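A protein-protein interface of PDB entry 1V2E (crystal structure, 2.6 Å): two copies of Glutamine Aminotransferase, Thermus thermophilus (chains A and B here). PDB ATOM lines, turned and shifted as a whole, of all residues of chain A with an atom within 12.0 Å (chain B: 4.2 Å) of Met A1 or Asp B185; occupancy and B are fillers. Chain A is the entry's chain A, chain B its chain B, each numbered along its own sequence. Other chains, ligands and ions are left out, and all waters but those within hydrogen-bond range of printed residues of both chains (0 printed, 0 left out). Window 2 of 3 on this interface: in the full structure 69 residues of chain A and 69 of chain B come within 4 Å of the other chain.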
ATOM      1  N   MET A   1      21.405 -10.829 -20.857  1.00  0.00           N
ATOM      2  CA  MET A   1      21.309  -9.409 -21.293  1.00  0.00           C
ATOM      3  C   MET A   1      20.001  -8.764 -20.863  1.00  0.00           C
ATOM      4  O   MET A   1      18.929  -9.218 -21.250  1.00  0.00           O
ATOM      5  CB  MET A   1      21.429  -9.332 -22.810  1.00  0.00           C
ATOM      6  CG  MET A   1      20.474 -10.251 -23.548  1.00  0.00           C
ATOM      7  SD  MET A   1      20.656 -10.159 -25.340  1.00  0.00           S
ATOM      8  CE  MET A   1      22.378  -9.606 -25.483  1.00  0.00           C
ATOM      9  N   ARG A   2      20.088  -7.712 -20.055  1.00  0.00           N
ATOM     10  CA  ARG A   2      18.895  -7.007 -19.604  1.00  0.00           C
ATOM     11  C   ARG A   2      19.058  -5.523 -19.902  1.00  0.00           C
ATOM     12  O   ARG A   2      20.176  -5.012 -19.953  1.00  0.00           O
ATOM     13  CB  ARG A   2      18.649  -7.235 -18.102  1.00  0.00           C
ATOM     14  CG  ARG A   2      19.459  -6.373 -17.133  1.00  0.00           C
ATOM     15  CD  ARG A   2      20.953  -6.693 -17.169  1.00  0.00           C
ATOM     16  NE  ARG A   2      21.704  -6.030 -16.099  1.00  0.00           N
ATOM     17  CZ  ARG A   2      21.734  -4.714 -15.895  1.00  0.00           C
ATOM     18  NH1 ARG A   2      21.049  -3.900 -16.690  1.00  0.00           N
ATOM     19  NH2 ARG A   2      22.451  -4.208 -14.897  1.00  0.00           N
ATOM     20  N   LEU A   3      17.946  -4.833 -20.124  1.00  0.00           N
ATOM     21  CA  LEU A   3      17.997  -3.406 -20.423  1.00  0.00           C
ATOM     22  C   LEU A   3      18.557  -2.638 -19.233  1.00  0.00           C
ATOM     23  O   LEU A   3      18.542  -3.123 -18.107  1.00  0.00           O
ATOM     24  CB  LEU A   3      16.594  -2.873 -20.720  1.00  0.00           C
ATOM     25  CG  LEU A   3      15.762  -3.435 -21.867  1.00  0.00           C
ATOM     26  CD1 LEU A   3      14.368  -2.846 -21.763  1.00  0.00           C
ATOM     27  CD2 LEU A   3      16.398  -3.114 -23.201  1.00  0.00           C
ATOM     28  N   HIS A   4      19.040  -1.430 -19.478  1.00  0.00           N
ATOM     29  CA  HIS A   4      19.563  -0.618 -18.393  1.00  0.00           C
ATOM     30  C   HIS A   4      18.390  -0.257 -17.472  1.00  0.00           C
ATOM     31  O   HIS A   4      17.282  -0.012 -17.942  1.00  0.00           O
ATOM     32  CB  HIS A   4      20.199   0.645 -18.955  1.00  0.00           C
ATOM     33  CG  HIS A   4      20.860   1.494 -17.920  1.00  0.00           C
ATOM     34  ND1 HIS A   4      20.154   2.164 -16.944  1.00  0.00           N
ATOM     35  CD2 HIS A   4      22.167   1.776 -17.703  1.00  0.00           C
ATOM     36  CE1 HIS A   4      20.998   2.824 -16.172  1.00  0.00           C
ATOM     37  NE2 HIS A   4      22.226   2.605 -16.611  1.00  0.00           N
ATOM     38  N   PRO A   5      18.619  -0.216 -16.150  1.00  0.00           N
ATOM     39  CA  PRO A   5      17.554   0.116 -15.191  1.00  0.00           C
ATOM     40  C   PRO A   5      16.763   1.394 -15.521  1.00  0.00           C
ATOM     41  O   PRO A   5      15.581   1.514 -15.168  1.00  0.00           O
ATOM     42  CB  PRO A   5      18.307   0.234 -13.866  1.00  0.00           C
ATOM     43  CG  PRO A   5      19.459  -0.729 -14.049  1.00  0.00           C
ATOM     44  CD  PRO A   5      19.902  -0.439 -15.458  1.00  0.00           C
ATOM     45  N   THR A   7      15.445   2.343 -18.129  1.00  0.00           N
ATOM     46  CA  THR A   7      14.265   2.005 -18.904  1.00  0.00           C
ATOM     47  C   THR A   7      13.091   1.597 -18.030  1.00  0.00           C
ATOM     48  O   THR A   7      12.084   1.114 -18.531  1.00  0.00           O
ATOM     49  CB  THR A   7      14.538   0.862 -19.879  1.00  0.00           C
ATOM     50  OG1 THR A   7      14.770  -0.344 -19.142  1.00  0.00           O
ATOM     51  CG2 THR A   7      15.745   1.179 -20.747  1.00  0.00           C
ATOM     52  N   ALA B 181      29.339 -11.326 -30.361  1.00  0.00           N
ATOM     53  CA  ALA B 181      28.179 -10.855 -29.623  1.00  0.00           C
ATOM     54  C   ALA B 181      27.509 -11.927 -28.768  1.00  0.00           C
ATOM     55  O   ALA B 181      27.188 -11.685 -27.604  1.00  0.00           O
ATOM     56  CB  ALA B 181      27.173 -10.249 -30.592  1.00  0.00           C
ATOM     57  N   ARG B 182      27.295 -13.107 -29.339  1.00  0.00           N
ATOM     58  CA  ARG B 182      26.648 -14.194 -28.605  1.00  0.00           C
ATOM     59  C   ARG B 182      27.569 -14.730 -27.498  1.00  0.00           C
ATOM     60  O   ARG B 182      27.115 -15.042 -26.393  1.00  0.00           O
ATOM     61  CB  ARG B 182      26.264 -15.332 -29.568  1.00  0.00           C
ATOM     62  CG  ARG B 182      25.918 -14.862 -30.979  1.00  0.00           C
ATOM     63  CD  ARG B 182      25.392 -15.985 -31.880  1.00  0.00           C
ATOM     64  NE  ARG B 182      23.931 -16.053 -31.882  1.00  0.00           N
ATOM     65  CZ  ARG B 182      23.206 -16.655 -32.824  1.00  0.00           C
ATOM     66  NH1 ARG B 182      21.880 -16.665 -32.743  1.00  0.00           N
ATOM     67  NH2 ARG B 182      23.806 -17.241 -33.849  1.00  0.00           N
ATOM     68  N   ALA B 183      28.862 -14.826 -27.799  1.00  0.00           N
ATOM     69  CA  ALA B 183      29.842 -15.325 -26.838  1.00  0.00           C
ATOM     70  C   ALA B 183      29.868 -14.456 -25.580  1.00  0.00           C
ATOM     71  O   ALA B 183      29.672 -14.947 -24.462  1.00  0.00           O
ATOM     72  CB  ALA B 183      31.226 -15.358 -27.486  1.00  0.00           C
ATOM     73  N   HIS B 184      30.101 -13.160 -25.778  1.00  0.00           N
ATOM     74  CA  HIS B 184      30.166 -12.192 -24.684  1.00  0.00           C
ATOM     75  C   HIS B 184      28.790 -11.713 -24.199  1.00  0.00           C
ATOM     76  O   HIS B 184      28.700 -10.910 -23.265  1.00  0.00           O
ATOM     77  CB  HIS B 184      31.011 -10.992 -25.119  1.00  0.00           C
ATOM     78  CG  HIS B 184      32.447 -11.331 -25.380  1.00  0.00           C
ATOM     79  ND1 HIS B 184      32.829 -12.358 -26.218  1.00  0.00           N
ATOM     80  CD2 HIS B 184      33.593 -10.770 -24.927  1.00  0.00           C
ATOM     81  CE1 HIS B 184      34.148 -12.415 -26.270  1.00  0.00           C
ATOM     82  NE2 HIS B 184      34.636 -11.461 -25.497  1.00  0.00           N
ATOM     83  N   ASP B 185      27.729 -12.214 -24.830  1.00  0.00           N
ATOM     84  CA  ASP B 185      26.356 -11.851 -24.477  1.00  0.00           C
ATOM     85  C   ASP B 185      26.101 -10.349 -24.645  1.00  0.00           C
ATOM     86  O   ASP B 185      25.525  -9.698 -23.770  1.00  0.00           O
ATOM     87  CB  ASP B 185      26.049 -12.275 -23.038  1.00  0.00           C
ATOM     88  CG  ASP B 185      24.563 -12.274 -22.740  1.00  0.00           C
ATOM     89  OD1 ASP B 185      23.804 -12.851 -23.550  1.00  0.00           O
ATOM     90  OD2 ASP B 185      24.148 -11.710 -21.700  1.00  0.00           O
ATOM     91  N   LEU B 186      26.533  -9.815 -25.783  1.00  0.00           N
ATOM     92  CA  LEU B 186      26.380  -8.397 -26.102  1.00  0.00           C
ATOM     93  C   LEU B 186      25.150  -8.102 -26.966  1.00  0.00           C
ATOM     94  O   LEU B 186      24.532  -9.012 -27.534  1.00  0.00           O
ATOM     95  CB  LEU B 186      27.590  -7.897 -26.887  1.00  0.00           C
ATOM     96  CG  LEU B 186      29.020  -7.946 -26.372  1.00  0.00           C
ATOM     97  CD1 LEU B 186      29.928  -7.435 -27.479  1.00  0.00           C
ATOM     98  CD2 LEU B 186      29.167  -7.097 -25.124  1.00  0.00           C
ATOM     99  N   PHE B 187      24.831  -6.811 -27.071  1.00  0.00           N
ATOM    100  CA  PHE B 187      23.731  -6.326 -27.902  1.00  0.00           C
ATOM    101  C   PHE B 187      24.345  -5.862 -29.206  1.00  0.00           C
ATOM    102  O   PHE B 187      25.478  -5.380 -29.223  1.00  0.00           O
ATOM    103  CB  PHE B 187      23.037  -5.130 -27.263  1.00  0.00           C
ATOM    104  CG  PHE B 187      21.993  -5.497 -26.276  1.00  0.00           C
ATOM    105  CD1 PHE B 187      20.926  -6.304 -26.650  1.00  0.00           C
ATOM    106  CD2 PHE B 187      22.063  -5.037 -24.970  1.00  0.00           C
ATOM    107  CE1 PHE B 187      19.941  -6.648 -25.734  1.00  0.00           C
ATOM    108  CE2 PHE B 187      21.086  -5.375 -24.045  1.00  0.00           C
ATOM    109  CZ  PHE B 187      20.024  -6.181 -24.428  1.00  0.00           C
ATOM    110  N   ARG B 213      19.439 -10.709 -30.414  1.00  0.00           N
ATOM    111  CA  ARG B 213      20.025  -9.579 -29.703  1.00  0.00           C
ATOM    112  C   ARG B 213      20.391  -8.412 -30.631  1.00  0.00           C
ATOM    113  O   ARG B 213      21.062  -7.471 -30.213  1.00  0.00           O
ATOM    114  CB  ARG B 213      21.273 -10.048 -28.944  1.00  0.00           C
ATOM    115  CG  ARG B 213      22.408 -10.484 -29.860  1.00  0.00           C
ATOM    116  CD  ARG B 213      23.575 -11.140 -29.115  1.00  0.00           C
ATOM    117  NE  ARG B 213      23.336 -12.546 -28.789  1.00  0.00           N
ATOM    118  CZ  ARG B 213      23.130 -13.011 -27.559  1.00  0.00           C
ATOM    119  NH1 ARG B 213      23.130 -12.181 -26.523  1.00  0.00           N
ATOM    120  NH2 ARG B 213      22.927 -14.311 -27.366  1.00  0.00           N
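The backbone carbonyl oxygen (O) of Ala B181 sits at hydrogen-bond distance from the backbone NH (N) of Leu B186 (2.7 Å).
The guanidinium group of Arg B213 is in salt-bridge range of the side-chain carboxylate of Asp B185 (3.1 Å).
Of chain B, only Asp B185, Leu B186, Phe B187 and Arg B213 come within 4 Å of Met A1.
Leu A3 touches none of the printed residues of chain B.
Ala B181 touches none of the printed residues of chain A.
Of the printed residues of chain A, Asp B185 touches Met A1 (3.0 Å).
Of chain A, only Met A1 (3.0 Å) comes within 4 Å of Leu B186.
The nearest residue of chain A that does not touch Asp B185 is Arg A2 (5.9 Å).
Among the printed residues, pairs that only touch across the chains: Met A1 with Leu B186 (3.0 Å) and Met A1 with Phe B187 (3.6 Å).
Printed residues of chain A that touch a printed residue of chain B: Met A1.
Hydrophobic or aromatic side chains of chain A that line the printed part of chain B: Met A1.
Among the printed residues, 4 pairs touch across the chains.
Among the printed residues, no Asp or Glu carboxylate lies within 4 Å of a Lys or Arg side-chain nitrogen of the other chain.
No position is printed for both chains.
The backbone NH (N) of Met A1 sits at hydrogen-bond distance from the side-chain carboxylate (OD2) of Asp B185 (3.0 Å).
The guanidinium group (NH1) of Arg B213 lies close to the side-chain sulfur (SD) of Met A1 (3.4 Å).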
